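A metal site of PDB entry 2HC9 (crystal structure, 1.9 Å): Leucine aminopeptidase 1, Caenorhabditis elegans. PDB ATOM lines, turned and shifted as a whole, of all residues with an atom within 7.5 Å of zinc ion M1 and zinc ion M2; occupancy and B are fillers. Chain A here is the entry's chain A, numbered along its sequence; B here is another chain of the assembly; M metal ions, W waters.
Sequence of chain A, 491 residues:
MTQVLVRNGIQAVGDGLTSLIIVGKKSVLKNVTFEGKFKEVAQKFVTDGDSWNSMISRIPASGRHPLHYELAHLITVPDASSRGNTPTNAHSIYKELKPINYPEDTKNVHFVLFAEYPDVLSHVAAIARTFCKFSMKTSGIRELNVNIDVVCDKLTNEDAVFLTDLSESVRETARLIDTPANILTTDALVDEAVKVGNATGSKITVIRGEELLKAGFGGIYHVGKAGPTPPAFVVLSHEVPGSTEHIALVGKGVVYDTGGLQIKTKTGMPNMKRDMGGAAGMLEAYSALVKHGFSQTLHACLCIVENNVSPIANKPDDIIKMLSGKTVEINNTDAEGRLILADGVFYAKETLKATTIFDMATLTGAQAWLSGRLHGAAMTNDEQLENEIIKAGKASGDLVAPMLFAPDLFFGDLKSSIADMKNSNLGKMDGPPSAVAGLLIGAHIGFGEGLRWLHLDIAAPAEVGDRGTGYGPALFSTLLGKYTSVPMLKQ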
ATOM      1  N   LYS A 252     -12.658 -25.123  -4.507  1.00  0.00           N
ATOM      2  CA  LYS A 252     -13.368 -25.632  -3.319  1.00  0.00           C
ATOM      3  C   LYS A 252     -13.820 -27.065  -3.551  1.00  0.00           C
ATOM      4  O   LYS A 252     -14.662 -27.325  -4.438  1.00  0.00           O
ATOM      5  CB  LYS A 252     -14.619 -24.780  -3.018  1.00  0.00           C
ATOM      6  CG  LYS A 252     -15.489 -25.327  -1.840  1.00  0.00           C
ATOM      7  CD  LYS A 252     -16.729 -24.456  -1.619  1.00  0.00           C
ATOM      8  CE  LYS A 252     -17.613 -25.138  -0.554  1.00  0.00           C
ATOM      9  NZ  LYS A 252     -18.874 -24.341  -0.235  1.00  0.00           N
ATOM     10  N   VAL A 254     -15.365 -29.424  -1.362  1.00  0.00           N
ATOM     11  CA  VAL A 254     -16.144 -29.983  -0.264  1.00  0.00           C
ATOM     12  C   VAL A 254     -16.952 -31.163  -0.803  1.00  0.00           C
ATOM     13  O   VAL A 254     -17.975 -30.989  -1.466  1.00  0.00           O
ATOM     14  CB  VAL A 254     -17.041 -28.914   0.409  1.00  0.00           C
ATOM     15  CG1 VAL A 254     -17.913 -29.573   1.498  1.00  0.00           C
ATOM     16  CG2 VAL A 254     -16.134 -27.806   1.047  1.00  0.00           C
ATOM     17  N   TYR A 256     -18.776 -33.369   0.564  1.00  0.00           N
ATOM     18  CA  TYR A 256     -20.164 -33.275   1.021  1.00  0.00           C
ATOM     19  C   TYR A 256     -20.246 -32.215   2.070  1.00  0.00           C
ATOM     20  O   TYR A 256     -19.373 -32.122   2.918  1.00  0.00           O
ATOM     21  CB  TYR A 256     -20.644 -34.599   1.638  1.00  0.00           C
ATOM     22  CG  TYR A 256     -22.136 -34.632   1.715  1.00  0.00           C
ATOM     23  CD1 TYR A 256     -22.900 -35.046   0.616  1.00  0.00           C
ATOM     24  CD2 TYR A 256     -22.811 -34.209   2.867  1.00  0.00           C
ATOM     25  CE1 TYR A 256     -24.287 -35.071   0.670  1.00  0.00           C
ATOM     26  CE2 TYR A 256     -24.183 -34.240   2.944  1.00  0.00           C
ATOM     27  CZ  TYR A 256     -24.911 -34.656   1.856  1.00  0.00           C
ATOM     28  OH  TYR A 256     -26.262 -34.663   1.978  1.00  0.00           O
ATOM     29  N   ASP A 257     -21.321 -31.431   2.015  1.00  0.00           N
ATOM     30  CA  ASP A 257     -21.538 -30.389   3.016  1.00  0.00           C
ATOM     31  C   ASP A 257     -22.860 -30.661   3.774  1.00  0.00           C
ATOM     32  O   ASP A 257     -23.943 -30.390   3.278  1.00  0.00           O
ATOM     33  CB  ASP A 257     -21.607 -29.040   2.304  1.00  0.00           C
ATOM     34  CG  ASP A 257     -21.514 -27.866   3.253  1.00  0.00           C
ATOM     35  OD1 ASP A 257     -21.336 -28.085   4.485  1.00  0.00           O
ATOM     36  OD2 ASP A 257     -21.615 -26.730   2.737  1.00  0.00           O
ATOM     37  N   THR A 258     -22.752 -31.195   4.996  1.00  0.00           N
ATOM     38  CA  THR A 258     -23.934 -31.306   5.869  1.00  0.00           C
ATOM     39  C   THR A 258     -24.306 -29.953   6.493  1.00  0.00           C
ATOM     40  O   THR A 258     -25.360 -29.829   7.121  1.00  0.00           O
ATOM     41  CB  THR A 258     -23.686 -32.244   7.057  1.00  0.00           C
ATOM     42  OG1 THR A 258     -22.683 -31.661   7.891  1.00  0.00           O
ATOM     43  CG2 THR A 258     -23.237 -33.655   6.601  1.00  0.00           C
ATOM     44  N   GLY A 259     -23.419 -28.964   6.327  1.00  0.00           N
ATOM     45  CA  GLY A 259     -23.531 -27.675   7.015  1.00  0.00           C
ATOM     46  C   GLY A 259     -22.669 -27.614   8.285  1.00  0.00           C
ATOM     47  O   GLY A 259     -22.330 -26.532   8.791  1.00  0.00           O
ATOM     48  N   GLY A 260     -22.331 -28.798   8.806  1.00  0.00           N
ATOM     49  CA  GLY A 260     -21.628 -28.892  10.095  1.00  0.00           C
ATOM     50  C   GLY A 260     -22.592 -28.803  11.251  1.00  0.00           C
ATOM     51  O   GLY A 260     -23.797 -29.049  11.095  1.00  0.00           O
ATOM     52  N   GLN A 262     -23.955 -26.327  12.666  1.00  0.00           N
ATOM     53  CA  GLN A 262     -25.076 -25.501  12.186  1.00  0.00           C
ATOM     54  C   GLN A 262     -25.634 -26.170  10.930  1.00  0.00           C
ATOM     55  O   GLN A 262     -25.392 -25.743   9.799  1.00  0.00           O
ATOM     56  CB  GLN A 262     -24.662 -24.048  11.947  1.00  0.00           C
ATOM     57  CG  GLN A 262     -24.441 -23.308  13.293  1.00  0.00           C
ATOM     58  CD  GLN A 262     -23.583 -22.097  13.127  1.00  0.00           C
ATOM     59  OE1 GLN A 262     -22.382 -22.213  12.845  1.00  0.00           O
ATOM     60  NE2 GLN A 262     -24.171 -20.920  13.292  1.00  0.00           N
ATOM     61  N   LYS A 264     -27.552 -28.148   7.879  1.00  0.00           N
ATOM     62  CA  LYS A 264     -28.534 -27.841   6.844  1.00  0.00           C
ATOM     63  C   LYS A 264     -29.881 -28.492   7.139  1.00  0.00           C
ATOM     64  O   LYS A 264     -29.980 -29.431   7.956  1.00  0.00           O
ATOM     65  CB  LYS A 264     -28.003 -28.286   5.478  1.00  0.00           C
ATOM     66  CG  LYS A 264     -26.770 -27.456   5.071  1.00  0.00           C
ATOM     67  CD  LYS A 264     -26.317 -27.916   3.656  1.00  0.00           C
ATOM     68  CE  LYS A 264     -25.082 -27.118   3.197  1.00  0.00           C
ATOM     69  NZ  LYS A 264     -25.477 -25.668   2.860  1.00  0.00           N
ATOM     70  N   MET A 272     -25.936 -31.778  -1.750  1.00  0.00           N
ATOM     71  CA  MET A 272     -24.669 -31.298  -1.218  1.00  0.00           C
ATOM     72  C   MET A 272     -23.405 -32.135  -1.524  1.00  0.00           C
ATOM     73  O   MET A 272     -22.301 -31.713  -1.195  1.00  0.00           O
ATOM     74  CB  MET A 272     -24.764 -30.969   0.284  1.00  0.00           C
ATOM     75  CG  MET A 272     -25.651 -29.739   0.587  1.00  0.00           C
ATOM     76  SD  MET A 272     -25.052 -28.245  -0.243  1.00  0.00           S
ATOM     77  CE  MET A 272     -26.148 -28.115  -1.630  1.00  0.00           C
ATOM     78  N   ASP A 275     -20.995 -29.894  -3.700  1.00  0.00           N
ATOM     79  CA  ASP A 275     -20.238 -28.792  -3.114  1.00  0.00           C
ATOM     80  C   ASP A 275     -18.709 -28.833  -3.399  1.00  0.00           C
ATOM     81  O   ASP A 275     -17.939 -28.023  -2.863  1.00  0.00           O
ATOM     82  CB  ASP A 275     -20.505 -28.749  -1.602  1.00  0.00           C
ATOM     83  CG  ASP A 275     -20.384 -27.359  -1.020  1.00  0.00           C
ATOM     84  OD1 ASP A 275     -20.614 -26.345  -1.717  1.00  0.00           O
ATOM     85  OD2 ASP A 275     -20.083 -27.295   0.182  1.00  0.00           O
ATOM     86  N   MET A 276     -18.289 -29.791  -4.216  1.00  0.00           N
ATOM     87  CA  MET A 276     -16.902 -29.881  -4.706  1.00  0.00           C
ATOM     88  C   MET A 276     -16.806 -29.495  -6.194  1.00  0.00           C
ATOM     89  O   MET A 276     -15.766 -29.739  -6.845  1.00  0.00           O
ATOM     90  CB  MET A 276     -16.339 -31.328  -4.486  1.00  0.00           C
ATOM     91  CG  MET A 276     -17.320 -32.502  -4.765  1.00  0.00           C
ATOM     92  SD  MET A 276     -18.123 -32.475  -6.369  1.00  0.00           S
ATOM     93  CE  MET A 276     -16.655 -32.850  -7.375  1.00  0.00           C
ATOM     94  N   ASN A 307     -17.503 -31.797   5.296  1.00  0.00           N
ATOM     95  CA  ASN A 307     -17.993 -30.970   6.409  1.00  0.00           C
ATOM     96  C   ASN A 307     -19.134 -31.733   7.110  1.00  0.00           C
ATOM     97  O   ASN A 307     -20.260 -31.779   6.593  1.00  0.00           O
ATOM     98  CB  ASN A 307     -18.465 -29.601   5.868  1.00  0.00           C
ATOM     99  CG  ASN A 307     -18.658 -28.560   6.975  1.00  0.00           C
ATOM    100  OD1 ASN A 307     -17.997 -28.629   8.013  1.00  0.00           O
ATOM    101  ND2 ASN A 307     -19.583 -27.630   6.767  1.00  0.00           N
ATOM    102  N   ASN A 332     -20.366 -19.450  11.631  1.00  0.00           N
ATOM    103  CA  ASN A 332     -21.195 -20.217  10.723  1.00  0.00           C
ATOM    104  C   ASN A 332     -20.394 -21.398  10.161  1.00  0.00           C
ATOM    105  O   ASN A 332     -19.570 -21.248   9.261  1.00  0.00           O
ATOM    106  CB  ASN A 332     -21.736 -19.326   9.592  1.00  0.00           C
ATOM    107  CG  ASN A 332     -22.723 -20.054   8.701  1.00  0.00           C
ATOM    108  OD1 ASN A 332     -22.944 -21.261   8.827  1.00  0.00           O
ATOM    109  ND2 ASN A 332     -23.315 -19.314   7.778  1.00  0.00           N
ATOM    110  N   THR A 333     -20.652 -22.579  10.689  1.00  0.00           N
ATOM    111  CA  THR A 333     -19.945 -23.796  10.264  1.00  0.00           C
ATOM    112  C   THR A 333     -20.271 -24.174   8.839  1.00  0.00           C
ATOM    113  O   THR A 333     -19.527 -24.951   8.248  1.00  0.00           O
ATOM    114  CB  THR A 333     -20.264 -25.021  11.165  1.00  0.00           C
ATOM    115  OG1 THR A 333     -21.662 -25.338  11.063  1.00  0.00           O
ATOM    116  CG2 THR A 333     -19.877 -24.713  12.635  1.00  0.00           C
ATOM    117  N   ASP A 334     -21.366 -23.647   8.290  1.00  0.00           N
ATOM    118  CA  ASP A 334     -21.770 -23.904   6.887  1.00  0.00           C
ATOM    119  C   ASP A 334     -21.112 -22.885   5.920  1.00  0.00           C
ATOM    120  O   ASP A 334     -21.248 -22.981   4.697  1.00  0.00           O
ATOM    121  CB  ASP A 334     -23.295 -23.808   6.795  1.00  0.00           C
ATOM    122  CG  ASP A 334     -23.874 -24.468   5.547  1.00  0.00           C
ATOM    123  OD1 ASP A 334     -23.131 -25.081   4.732  1.00  0.00           O
ATOM    124  OD2 ASP A 334     -25.095 -24.384   5.376  1.00  0.00           O
ATOM    125  N   ALA A 335     -20.411 -21.896   6.469  1.00  0.00           N
ATOM    126  CA  ALA A 335     -19.631 -20.968   5.648  1.00  0.00           C
ATOM    127  C   ALA A 335     -18.185 -21.501   5.632  1.00  0.00           C
ATOM    128  O   ALA A 335     -17.205 -20.800   5.995  1.00  0.00           O
ATOM    129  CB  ALA A 335     -19.711 -19.538   6.258  1.00  0.00           C
ATOM    130  N   GLU A 336     -18.070 -22.772   5.223  1.00  0.00           N
ATOM    131  CA  GLU A 336     -16.811 -23.528   5.365  1.00  0.00           C
ATOM    132  C   GLU A 336     -15.918 -23.427   4.124  1.00  0.00           C
ATOM    133  O   GLU A 336     -14.663 -23.507   4.230  1.00  0.00           O
ATOM    134  CB  GLU A 336     -17.086 -25.004   5.749  1.00  0.00           C
ATOM    135  CG  GLU A 336     -17.283 -25.960   4.537  1.00  0.00           C
ATOM    136  CD  GLU A 336     -18.557 -25.674   3.772  1.00  0.00           C
ATOM    137  OE1 GLU A 336     -18.612 -25.914   2.545  1.00  0.00           O
ATOM    138  OE2 GLU A 336     -19.528 -25.197   4.388  1.00  0.00           O
ATOM    139  N   GLY A 337     -16.531 -23.265   2.950  1.00  0.00           N
ATOM    140  CA  GLY A 337     -15.754 -23.128   1.707  1.00  0.00           C
ATOM    141  C   GLY A 337     -14.777 -21.953   1.764  1.00  0.00           C
ATOM    142  O   GLY A 337     -13.628 -22.068   1.344  1.00  0.00           O
ATOM    143  N   ARG A 338     -15.225 -20.848   2.311  1.00  0.00           N
ATOM    144  CA  ARG A 338     -14.399 -19.656   2.341  1.00  0.00           C
ATOM    145  C   ARG A 338     -13.193 -19.834   3.291  1.00  0.00           C
ATOM    146  O   ARG A 338     -12.123 -19.278   3.038  1.00  0.00           O
ATOM    147  CB  ARG A 338     -15.228 -18.417   2.704  1.00  0.00           C
ATOM    148  CG  ARG A 338     -15.816 -18.465   4.150  1.00  0.00           C
ATOM    149  CD  ARG A 338     -16.928 -17.394   4.316  1.00  0.00           C
ATOM    150  NE  ARG A 338     -18.165 -17.835   3.645  1.00  0.00           N
ATOM    151  CZ  ARG A 338     -19.321 -17.180   3.738  1.00  0.00           C
ATOM    152  NH1 ARG A 338     -19.404 -16.075   4.497  1.00  0.00           N
ATOM    153  NH2 ARG A 338     -20.398 -17.653   3.120  1.00  0.00           N
ATOM    154  N   ILE A 340     -11.612 -22.812   3.846  1.00  0.00           N
ATOM    155  CA  ILE A 340     -10.616 -23.657   3.194  1.00  0.00           C
ATOM    156  C   ILE A 340      -9.914 -22.916   2.055  1.00  0.00           C
ATOM    157  O   ILE A 340      -8.700 -23.106   1.840  1.00  0.00           O
ATOM    158  CB  ILE A 340     -11.174 -25.050   2.790  1.00  0.00           C
ATOM    159  CG1 ILE A 340     -12.096 -24.945   1.560  1.00  0.00           C
ATOM    160  CG2 ILE A 340     -11.916 -25.706   3.995  1.00  0.00           C
ATOM    161  CD1 ILE A 340     -12.627 -26.331   1.038  1.00  0.00           C
ATOM    162  N   THR A 362     -18.457 -23.480  -5.419  1.00  0.00           N
ATOM    163  CA  THR A 362     -19.915 -23.463  -5.221  1.00  0.00           C
ATOM    164  C   THR A 362     -20.149 -22.887  -3.822  1.00  0.00           C
ATOM    165  O   THR A 362     -20.316 -23.629  -2.849  1.00  0.00           O
ATOM    166  CB  THR A 362     -20.506 -24.901  -5.305  1.00  0.00           C
ATOM    167  OG1 THR A 362     -19.795 -25.746  -4.409  1.00  0.00           O
ATOM    168  CG2 THR A 362     -20.344 -25.451  -6.702  1.00  0.00           C
ATOM    169  N   LEU A 363     -20.096 -21.556  -3.695  1.00  0.00           N
ATOM    170  CA  LEU A 363     -19.836 -20.976  -2.391  1.00  0.00           C
ATOM    171  C   LEU A 363     -21.127 -20.657  -1.618  1.00  0.00           C
ATOM    172  O   LEU A 363     -21.240 -20.992  -0.443  1.00  0.00           O
ATOM    173  CB  LEU A 363     -18.909 -19.732  -2.473  1.00  0.00           C
ATOM    174  CG  LEU A 363     -18.233 -19.421  -1.129  1.00  0.00           C
ATOM    175  CD1 LEU A 363     -17.269 -20.544  -0.677  1.00  0.00           C
ATOM    176  CD2 LEU A 363     -17.482 -18.095  -1.239  1.00  0.00           C
ATOM    177  N   THR A 364     -22.084 -19.998  -2.274  1.00  0.00           N
ATOM    178  CA  THR A 364     -23.259 -19.430  -1.562  1.00  0.00           C
ATOM    179  C   THR A 364     -24.548 -19.649  -2.339  1.00  0.00           C
ATOM    180  O   THR A 364     -24.570 -19.523  -3.550  1.00  0.00           O
ATOM    181  CB  THR A 364     -23.096 -17.900  -1.290  1.00  0.00           C
ATOM    182  OG1 THR A 364     -23.027 -17.159  -2.537  1.00  0.00           O
ATOM    183  CG2 THR A 364     -21.823 -17.639  -0.475  1.00  0.00           C
ATOM    184  N   LYS B 266     -29.406 -22.655  13.599  1.00  0.00           N
ATOM    185  CA  LYS B 266     -28.268 -21.934  13.018  1.00  0.00           C
ATOM    186  C   LYS B 266     -27.983 -20.619  13.742  1.00  0.00           C
ATOM    187  O   LYS B 266     -26.820 -20.257  13.964  1.00  0.00           O
ATOM    188  CB  LYS B 266     -28.533 -21.646  11.541  1.00  0.00           C
ATOM    189  CG  LYS B 266     -27.368 -20.929  10.855  1.00  0.00           C
ATOM    190  CD  LYS B 266     -27.518 -20.997   9.338  1.00  0.00           C
ATOM    191  CE  LYS B 266     -26.189 -21.318   8.661  1.00  0.00           C
ATOM    192  NZ  LYS B 266     -26.271 -21.137   7.157  1.00  0.00           N
HETATM  193 ZN    ZN M   1     -21.437 -24.929   3.710  1.00  0.00          ZN
HETATM  194 ZN    ZN M   2     -20.009 -25.546   1.088  1.00  0.00          ZN
HETATM  195  O   HOH W   1     -21.258 -24.076   1.878  1.00  0.00           O
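Along chain A the residues within 4 Å of zinc ion M2 span positions 252 to 336. The nearest printed residue that does not touch zinc ion M2 is Thr 362 (4.4 Å).
The backbone carbonyl oxygen (O) of Gly 259 is in hydrogen-bond range of the backbone NH (N) of Asp 334 (3.1 Å). The backbone carbonyl oxygen (O) of Thr 362 lies close to the side-chain amino group (NZ) of Lys 252, at 3.1 Å. O of Asp 275 is in hydrogen-bond range of N of Val 254, at 3.3 Å. The backbone NH of Asp 257 sits at hydrogen-bond distance from the backbone carbonyl oxygen of Met 272. The side-chain carboxylate of Asp 257 sits at hydrogen-bond distance from the backbone NH of Gly 259. The side-chain carboxylate of Asp 275 lies within hydrogen-bond range of the side-chain hydroxyl of Thr 362 (2.9 Å). The backbone NH (N) of Asp 334 lies within hydrogen-bond range of the side-chain amide oxygen (OD1) of Asn 332. NZ of Lys 264 is in salt-bridge range of OD2 of Asp 334.
Zinc ion M1 is bound by the side-chain carboxylate (OD1) of Asp 334, water W1, the side-chain carboxylate (OE2) of Glu 336, the side-chain carboxylate (OD2) of Asp 257 and the backbone carbonyl oxygen (O) of Asp 334.
Zinc ion M2 is bound by the side-chain carboxylate of Asp 275 (2.0 Å), the side-chain carboxylate of Glu 336 (2.1 Å), water W1 (2.1 Å), the side-chain amino group of Lys 252 (2.1 Å) and the side-chain carboxylate of Asp 257 (2.6 Å). Zinc ion M2 has five donor atoms within binding distance.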
